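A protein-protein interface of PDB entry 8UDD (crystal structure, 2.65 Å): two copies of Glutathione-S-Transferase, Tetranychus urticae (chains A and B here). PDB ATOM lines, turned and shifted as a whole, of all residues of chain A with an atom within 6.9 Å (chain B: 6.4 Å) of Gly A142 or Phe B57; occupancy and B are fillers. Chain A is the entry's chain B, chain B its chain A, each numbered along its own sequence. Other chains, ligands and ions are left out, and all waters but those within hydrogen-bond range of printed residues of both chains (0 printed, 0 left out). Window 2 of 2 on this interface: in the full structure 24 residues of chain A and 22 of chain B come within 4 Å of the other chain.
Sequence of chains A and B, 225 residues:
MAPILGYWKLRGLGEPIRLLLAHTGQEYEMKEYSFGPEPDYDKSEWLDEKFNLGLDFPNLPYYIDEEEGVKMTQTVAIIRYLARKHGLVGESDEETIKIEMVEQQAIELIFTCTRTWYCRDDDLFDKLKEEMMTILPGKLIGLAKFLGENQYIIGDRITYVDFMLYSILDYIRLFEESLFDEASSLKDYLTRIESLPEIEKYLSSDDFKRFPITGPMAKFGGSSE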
ATOM      1  N   LYS A  98     -12.076 -17.193  -7.097  1.00  0.00           N
ATOM      2  CA  LYS A  98     -13.394 -17.685  -6.727  1.00  0.00           C
ATOM      3  C   LYS A  98     -14.380 -16.545  -6.453  1.00  0.00           C
ATOM      4  O   LYS A  98     -15.498 -16.569  -6.938  1.00  0.00           O
ATOM      5  CB  LYS A  98     -13.279 -18.571  -5.479  1.00  0.00           C
ATOM      6  CG  LYS A  98     -12.572 -19.921  -5.659  1.00  0.00           C
ATOM      7  CD  LYS A  98     -12.645 -20.721  -4.389  1.00  0.00           C
ATOM      8  CE  LYS A  98     -11.451 -21.617  -4.154  1.00  0.00           C
ATOM      9  NZ  LYS A  98     -11.129 -21.691  -2.705  1.00  0.00           N
ATOM     10  N   MET A 101     -15.256 -14.717  -9.818  1.00  0.00           N
ATOM     11  CA  MET A 101     -16.137 -15.543 -10.634  1.00  0.00           C
ATOM     12  C   MET A 101     -17.584 -15.436 -10.138  1.00  0.00           C
ATOM     13  O   MET A 101     -18.497 -15.245 -10.939  1.00  0.00           O
ATOM     14  CB  MET A 101     -15.716 -17.008 -10.589  1.00  0.00           C
ATOM     15  CG  MET A 101     -14.491 -17.268 -11.401  1.00  0.00           C
ATOM     16  SD  MET A 101     -14.439 -18.960 -11.985  1.00  0.00           S
ATOM     17  CE  MET A 101     -14.077 -19.869 -10.496  1.00  0.00           C
ATOM     18  N   VAL A 102     -17.773 -15.529  -8.814  1.00  0.00           N
ATOM     19  CA  VAL A 102     -19.090 -15.488  -8.204  1.00  0.00           C
ATOM     20  C   VAL A 102     -19.671 -14.073  -8.299  1.00  0.00           C
ATOM     21  O   VAL A 102     -20.892 -13.897  -8.430  1.00  0.00           O
ATOM     22  CB  VAL A 102     -19.044 -15.939  -6.731  1.00  0.00           C
ATOM     23  CG1 VAL A 102     -20.375 -15.645  -6.033  1.00  0.00           C
ATOM     24  CG2 VAL A 102     -18.648 -17.412  -6.577  1.00  0.00           C
ATOM     25  N   GLN A 105     -20.839 -14.103 -11.841  1.00  0.00           N
ATOM     26  CA  GLN A 105     -21.988 -14.987 -11.909  1.00  0.00           C
ATOM     27  C   GLN A 105     -23.221 -14.315 -11.276  1.00  0.00           C
ATOM     28  O   GLN A 105     -24.307 -14.402 -11.832  1.00  0.00           O
ATOM     29  CB  GLN A 105     -21.627 -16.340 -11.300  1.00  0.00           C
ATOM     30  CG  GLN A 105     -22.763 -17.329 -11.375  1.00  0.00           C
ATOM     31  CD  GLN A 105     -23.017 -17.770 -12.792  1.00  0.00           C
ATOM     32  OE1 GLN A 105     -22.410 -18.732 -13.262  1.00  0.00           O
ATOM     33  NE2 GLN A 105     -23.955 -17.105 -13.452  1.00  0.00           N
ATOM     34  N   LEU A 136     -32.560 -20.192 -15.382  1.00  0.00           N
ATOM     35  CA  LEU A 136     -32.173 -19.947 -14.000  1.00  0.00           C
ATOM     36  C   LEU A 136     -31.932 -21.244 -13.236  1.00  0.00           C
ATOM     37  O   LEU A 136     -31.021 -21.281 -12.419  1.00  0.00           O
ATOM     38  CB  LEU A 136     -33.238 -19.094 -13.311  1.00  0.00           C
ATOM     39  CG  LEU A 136     -33.068 -17.591 -13.513  1.00  0.00           C
ATOM     40  CD1 LEU A 136     -34.292 -16.810 -13.061  1.00  0.00           C
ATOM     41  CD2 LEU A 136     -31.847 -17.114 -12.761  1.00  0.00           C
ATOM     42  N   PRO A 137     -32.736 -22.319 -13.413  1.00  0.00           N
ATOM     43  CA  PRO A 137     -32.530 -23.546 -12.642  1.00  0.00           C
ATOM     44  C   PRO A 137     -31.111 -24.095 -12.750  1.00  0.00           C
ATOM     45  O   PRO A 137     -30.573 -24.564 -11.759  1.00  0.00           O
ATOM     46  CB  PRO A 137     -33.552 -24.527 -13.236  1.00  0.00           C
ATOM     47  CG  PRO A 137     -34.642 -23.624 -13.762  1.00  0.00           C
ATOM     48  CD  PRO A 137     -33.909 -22.411 -14.299  1.00  0.00           C
ATOM     49  N   GLY A 138     -30.522 -24.024 -13.950  1.00  0.00           N
ATOM     50  CA  GLY A 138     -29.185 -24.544 -14.217  1.00  0.00           C
ATOM     51  C   GLY A 138     -28.090 -23.669 -13.598  1.00  0.00           C
ATOM     52  O   GLY A 138     -27.058 -24.178 -13.132  1.00  0.00           O
ATOM     53  N   LYS A 139     -28.356 -22.352 -13.584  1.00  0.00           N
ATOM     54  CA  LYS A 139     -27.495 -21.366 -12.947  1.00  0.00           C
ATOM     55  C   LYS A 139     -27.506 -21.532 -11.422  1.00  0.00           C
ATOM     56  O   LYS A 139     -26.473 -21.438 -10.780  1.00  0.00           O
ATOM     57  CB  LYS A 139     -27.924 -19.961 -13.389  1.00  0.00           C
ATOM     58  N   LEU A 140     -28.670 -21.796 -10.834  1.00  0.00           N
ATOM     59  CA  LEU A 140     -28.790 -22.001  -9.393  1.00  0.00           C
ATOM     60  C   LEU A 140     -28.190 -23.346  -8.967  1.00  0.00           C
ATOM     61  O   LEU A 140     -27.587 -23.437  -7.898  1.00  0.00           O
ATOM     62  CB  LEU A 140     -30.271 -21.898  -9.010  1.00  0.00           C
ATOM     63  CG  LEU A 140     -30.911 -20.542  -9.299  1.00  0.00           C
ATOM     64  CD1 LEU A 140     -32.414 -20.584  -9.051  1.00  0.00           C
ATOM     65  CD2 LEU A 140     -30.250 -19.451  -8.475  1.00  0.00           C
ATOM     66  N   ILE A 141     -28.354 -24.388  -9.790  1.00  0.00           N
ATOM     67  CA  ILE A 141     -27.664 -25.642  -9.540  1.00  0.00           C
ATOM     68  C   ILE A 141     -26.144 -25.426  -9.545  1.00  0.00           C
ATOM     69  O   ILE A 141     -25.431 -25.966  -8.693  1.00  0.00           O
ATOM     70  CB  ILE A 141     -28.084 -26.711 -10.562  1.00  0.00           C
ATOM     71  CG1 ILE A 141     -29.460 -27.300 -10.237  1.00  0.00           C
ATOM     72  CG2 ILE A 141     -27.036 -27.810 -10.652  1.00  0.00           C
ATOM     73  CD1 ILE A 141     -30.140 -27.964 -11.420  1.00  0.00           C
ATOM     74  N   GLY A 142     -25.641 -24.648 -10.516  1.00  0.00           N
ATOM     75  CA  GLY A 142     -24.226 -24.337 -10.579  1.00  0.00           C
ATOM     76  C   GLY A 142     -23.695 -23.709  -9.292  1.00  0.00           C
ATOM     77  O   GLY A 142     -22.625 -24.101  -8.810  1.00  0.00           O
ATOM     78  N   LEU A 143     -24.447 -22.722  -8.769  1.00  0.00           N
ATOM     79  CA  LEU A 143     -24.095 -22.016  -7.544  1.00  0.00           C
ATOM     80  C   LEU A 143     -24.211 -22.954  -6.341  1.00  0.00           C
ATOM     81  O   LEU A 143     -23.362 -22.909  -5.453  1.00  0.00           O
ATOM     82  CB  LEU A 143     -25.000 -20.790  -7.371  1.00  0.00           C
ATOM     83  CG  LEU A 143     -24.648 -19.598  -8.272  1.00  0.00           C
ATOM     84  CD1 LEU A 143     -25.740 -18.527  -8.242  1.00  0.00           C
ATOM     85  CD2 LEU A 143     -23.300 -18.991  -7.889  1.00  0.00           C
ATOM     86  N   ALA A 144     -25.259 -23.788  -6.289  1.00  0.00           N
ATOM     87  CA  ALA A 144     -25.377 -24.756  -5.214  1.00  0.00           C
ATOM     88  C   ALA A 144     -24.142 -25.658  -5.188  1.00  0.00           C
ATOM     89  O   ALA A 144     -23.559 -25.863  -4.129  1.00  0.00           O
ATOM     90  CB  ALA A 144     -26.645 -25.549  -5.364  1.00  0.00           C
ATOM     91  N   LYS A 145     -23.757 -26.191  -6.356  1.00  0.00           N
ATOM     92  CA  LYS A 145     -22.598 -27.070  -6.476  1.00  0.00           C
ATOM     93  C   LYS A 145     -21.320 -26.321  -6.057  1.00  0.00           C
ATOM     94  O   LYS A 145     -20.387 -26.916  -5.546  1.00  0.00           O
ATOM     95  CB  LYS A 145     -22.497 -27.624  -7.903  1.00  0.00           C
ATOM     96  CG  LYS A 145     -21.877 -29.016  -8.035  1.00  0.00           C
ATOM     97  CD  LYS A 145     -21.349 -29.401  -9.434  1.00  0.00           C
ATOM     98  N   PHE A 146     -21.257 -25.013  -6.287  1.00  0.00           N
ATOM     99  CA  PHE A 146     -20.092 -24.237  -5.906  1.00  0.00           C
ATOM    100  C   PHE A 146     -20.020 -24.043  -4.382  1.00  0.00           C
ATOM    101  O   PHE A 146     -18.973 -24.216  -3.774  1.00  0.00           O
ATOM    102  CB  PHE A 146     -20.093 -22.876  -6.618  1.00  0.00           C
ATOM    103  CG  PHE A 146     -18.761 -22.177  -6.513  1.00  0.00           C
ATOM    104  CD1 PHE A 146     -17.653 -22.636  -7.217  1.00  0.00           C
ATOM    105  CD2 PHE A 146     -18.581 -21.154  -5.603  1.00  0.00           C
ATOM    106  CE1 PHE A 146     -16.415 -22.029  -7.057  1.00  0.00           C
ATOM    107  CE2 PHE A 146     -17.342 -20.549  -5.450  1.00  0.00           C
ATOM    108  CZ  PHE A 146     -16.263 -20.981  -6.180  1.00  0.00           C
ATOM    109  N   LEU A 147     -21.116 -23.592  -3.776  1.00  0.00           N
ATOM    110  CA  LEU A 147     -21.213 -23.425  -2.336  1.00  0.00           C
ATOM    111  C   LEU A 147     -20.869 -24.733  -1.615  1.00  0.00           C
ATOM    112  O   LEU A 147     -20.276 -24.710  -0.535  1.00  0.00           O
ATOM    113  CB  LEU A 147     -22.650 -22.983  -2.023  1.00  0.00           C
ATOM    114  CG  LEU A 147     -22.997 -22.717  -0.557  1.00  0.00           C
ATOM    115  CD1 LEU A 147     -22.262 -21.502   0.000  1.00  0.00           C
ATOM    116  CD2 LEU A 147     -24.496 -22.508  -0.419  1.00  0.00           C
ATOM    117  N   ILE A 153     -20.113 -18.585   0.371  1.00  0.00           N
ATOM    118  CA  ILE A 153     -19.751 -19.037  -1.009  1.00  0.00           C
ATOM    119  C   ILE A 153     -18.256 -19.355  -1.115  1.00  0.00           C
ATOM    120  O   ILE A 153     -17.915 -20.248  -1.900  1.00  0.00           O
ATOM    121  CB  ILE A 153     -20.204 -18.003  -2.060  1.00  0.00           C
ATOM    122  CG1 ILE A 153     -20.093 -18.554  -3.481  1.00  0.00           C
ATOM    123  CG2 ILE A 153     -19.456 -16.691  -1.895  1.00  0.00           C
ATOM    124  CD1 ILE A 153     -21.036 -19.697  -3.764  1.00  0.00           C
ATOM    125  N   ALA A 183     -32.222 -26.551  -5.796  1.00  0.00           N
ATOM    126  CA  ALA A 183     -31.049 -25.968  -5.104  1.00  0.00           C
ATOM    127  C   ALA A 183     -31.452 -25.524  -3.695  1.00  0.00           C
ATOM    128  O   ALA A 183     -31.457 -24.307  -3.443  1.00  0.00           O
ATOM    129  CB  ALA A 183     -30.508 -24.819  -5.912  1.00  0.00           C
ATOM    130  N   LYS B  50     -18.198 -28.727 -22.968  1.00  0.00           N
ATOM    131  CA  LYS B  50     -18.504 -27.751 -21.938  1.00  0.00           C
ATOM    132  C   LYS B  50     -18.311 -28.332 -20.524  1.00  0.00           C
ATOM    133  O   LYS B  50     -17.717 -27.693 -19.653  1.00  0.00           O
ATOM    134  CB  LYS B  50     -19.940 -27.291 -22.203  1.00  0.00           C
ATOM    135  CG  LYS B  50     -20.538 -26.401 -21.134  1.00  0.00           C
ATOM    136  CD  LYS B  50     -21.959 -25.946 -21.418  1.00  0.00           C
ATOM    137  CE  LYS B  50     -22.399 -24.887 -20.425  1.00  0.00           C
ATOM    138  NZ  LYS B  50     -23.581 -24.138 -20.905  1.00  0.00           N
ATOM    139  N   LEU B  55     -14.737 -26.922 -15.198  1.00  0.00           N
ATOM    140  CA  LEU B  55     -15.117 -25.544 -14.884  1.00  0.00           C
ATOM    141  C   LEU B  55     -16.305 -25.542 -13.930  1.00  0.00           C
ATOM    142  O   LEU B  55     -17.264 -26.270 -14.139  1.00  0.00           O
ATOM    143  CB  LEU B  55     -15.494 -24.785 -16.161  1.00  0.00           C
ATOM    144  CG  LEU B  55     -14.418 -24.686 -17.238  1.00  0.00           C
ATOM    145  CD1 LEU B  55     -14.997 -24.014 -18.470  1.00  0.00           C
ATOM    146  CD2 LEU B  55     -13.180 -23.949 -16.732  1.00  0.00           C
ATOM    147  N   ASP B  56     -16.243 -24.650 -12.942  1.00  0.00           N
ATOM    148  CA  ASP B  56     -17.282 -24.468 -11.940  1.00  0.00           C
ATOM    149  C   ASP B  56     -18.552 -23.912 -12.584  1.00  0.00           C
ATOM    150  O   ASP B  56     -19.661 -24.330 -12.237  1.00  0.00           O
ATOM    151  CB  ASP B  56     -16.785 -23.571 -10.806  1.00  0.00           C
ATOM    152  CG  ASP B  56     -15.603 -24.143 -10.039  1.00  0.00           C
ATOM    153  OD1 ASP B  56     -15.678 -25.317  -9.679  1.00  0.00           O
ATOM    154  OD2 ASP B  56     -14.623 -23.396  -9.768  1.00  0.00           O
ATOM    155  N   PHE B  57     -18.367 -22.894 -13.421  1.00  0.00           N
ATOM    156  CA  PHE B  57     -19.512 -22.259 -14.113  1.00  0.00           C
ATOM    157  C   PHE B  57     -19.217 -22.337 -15.609  1.00  0.00           C
ATOM    158  O   PHE B  57     -18.878 -21.308 -16.215  1.00  0.00           O
ATOM    159  CB  PHE B  57     -19.685 -20.820 -13.629  1.00  0.00           C
ATOM    160  CG  PHE B  57     -19.766 -20.661 -12.132  1.00  0.00           C
ATOM    161  CD1 PHE B  57     -20.806 -21.222 -11.412  1.00  0.00           C
ATOM    162  CD2 PHE B  57     -18.792 -19.958 -11.441  1.00  0.00           C
ATOM    163  CE1 PHE B  57     -20.877 -21.076 -10.037  1.00  0.00           C
ATOM    164  CE2 PHE B  57     -18.862 -19.815 -10.066  1.00  0.00           C
ATOM    165  CZ  PHE B  57     -19.905 -20.373  -9.366  1.00  0.00           C
ATOM    166  N   PRO B  58     -19.321 -23.528 -16.232  1.00  0.00           N
ATOM    167  CA  PRO B  58     -18.954 -23.681 -17.634  1.00  0.00           C
ATOM    168  C   PRO B  58     -19.543 -22.564 -18.501  1.00  0.00           C
ATOM    169  O   PRO B  58     -20.753 -22.442 -18.550  1.00  0.00           O
ATOM    170  CB  PRO B  58     -19.589 -25.032 -17.988  1.00  0.00           C
ATOM    171  CG  PRO B  58     -19.529 -25.807 -16.699  1.00  0.00           C
ATOM    172  CD  PRO B  58     -19.813 -24.771 -15.632  1.00  0.00           C
ATOM    173  N   ASN B  59     -18.678 -21.783 -19.152  1.00  0.00           N
ATOM    174  CA  ASN B  59     -19.146 -20.708 -20.067  1.00  0.00           C
ATOM    175  C   ASN B  59     -17.980 -20.283 -20.964  1.00  0.00           C
ATOM    176  O   ASN B  59     -16.832 -20.632 -20.638  1.00  0.00           O
ATOM    177  CB  ASN B  59     -19.713 -19.506 -19.308  1.00  0.00           C
ATOM    178  CG  ASN B  59     -20.701 -18.711 -20.133  1.00  0.00           C
ATOM    179  OD1 ASN B  59     -20.402 -18.326 -21.260  1.00  0.00           O
ATOM    180  ND2 ASN B  59     -21.888 -18.488 -19.594  1.00  0.00           N
ATOM    181  N   LEU B  60     -18.274 -19.579 -22.059  1.00  0.00           N
ATOM    182  CA  LEU B  60     -17.203 -19.054 -22.947  1.00  0.00           C
ATOM    183  C   LEU B  60     -17.195 -17.528 -22.828  1.00  0.00           C
ATOM    184  O   LEU B  60     -18.233 -16.912 -23.125  1.00  0.00           O
ATOM    185  CB  LEU B  60     -17.485 -19.494 -24.386  1.00  0.00           C
ATOM    186  CG  LEU B  60     -17.031 -20.907 -24.748  1.00  0.00           C
ATOM    187  CD1 LEU B  60     -17.162 -21.149 -26.244  1.00  0.00           C
ATOM    188  CD2 LEU B  60     -15.598 -21.140 -24.301  1.00  0.00           C
ATOM    189  N   THR B  73     -13.605 -18.989 -15.377  1.00  0.00           N
ATOM    190  CA  THR B  73     -14.603 -18.522 -16.369  1.00  0.00           C
ATOM    191  C   THR B  73     -14.878 -17.069 -15.977  1.00  0.00           C
ATOM    192  O   THR B  73     -14.179 -16.592 -15.069  1.00  0.00           O
ATOM    193  CB  THR B  73     -15.869 -19.386 -16.384  1.00  0.00           C
ATOM    194  OG1 THR B  73     -16.302 -19.567 -15.036  1.00  0.00           O
ATOM    195  CG2 THR B  73     -15.660 -20.731 -17.040  1.00  0.00           C
ATOM    196  N   GLN B  74     -15.827 -16.402 -16.632  1.00  0.00           N
ATOM    197  CA  GLN B  74     -16.181 -14.987 -16.325  1.00  0.00           C
ATOM    198  C   GLN B  74     -15.108 -14.054 -16.902  1.00  0.00           C
ATOM    199  O   GLN B  74     -14.010 -13.998 -16.329  1.00  0.00           O
ATOM    200  CB  GLN B  74     -16.431 -14.794 -14.826  1.00  0.00           C
ATOM    201  CG  GLN B  74     -17.477 -15.741 -14.253  1.00  0.00           C
ATOM    202  CD  GLN B  74     -18.770 -15.736 -15.031  1.00  0.00           C
ATOM    203  OE1 GLN B  74     -19.425 -14.707 -15.178  1.00  0.00           O
ATOM    204  NE2 GLN B  74     -19.150 -16.897 -15.535  1.00  0.00           N
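No position is printed for both chains. Of the 9 pairs that touch across the chains among the printed residues, none has its exchanged pair printed and touching as well.
Of the 18 printed residues of chain A, 5 touch a printed residue of chain B. Among the printed residues, 9 pairs touch across the chains.
Among the printed residues, pairs that only touch across the chains: Met A101 with Asp B56 (3.6 Å), Met A101 with Gln B74 (3.5 Å), Gln A105 with Phe B57 (3.5 Å), Gln A105 with Gln B74 (3.7 Å), Gly A142 with Phe B57 (3.7 Å), Leu A143 with Phe B57 (3.9 Å), Phe A146 with Asp B56 (3.5 Å) and Phe A146 with Phe B57 (3.6 Å).
The backbone carbonyl oxygen of Phe B57 sits at hydrogen-bond distance from the side-chain hydroxyl of Thr B73, 3.3 Å away.
N of Thr B73 is in hydrogen-bond range of SD of Met A101 (3.5 Å).
Gly A142 touches one residue of chain B. Of the printed residues of chain A, Phe B57 touches Gln A105, Gly A142, Leu A143 and Phe A146. Of the printed residues of chain B, Gln A105 touches Phe B57 (3.5 Å) and Gln B74 (3.7 Å). Printed residues of chain B within 4 Å of Met A101: Asp B56, Thr B73 and Gln B74. Ile A141 touches none of the printed residues of chain B. Leu A136 touches none of the printed residues of chain B. The nearest residue of chain B that does not touch Gly A142 is Asp B56 (4.5 Å).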
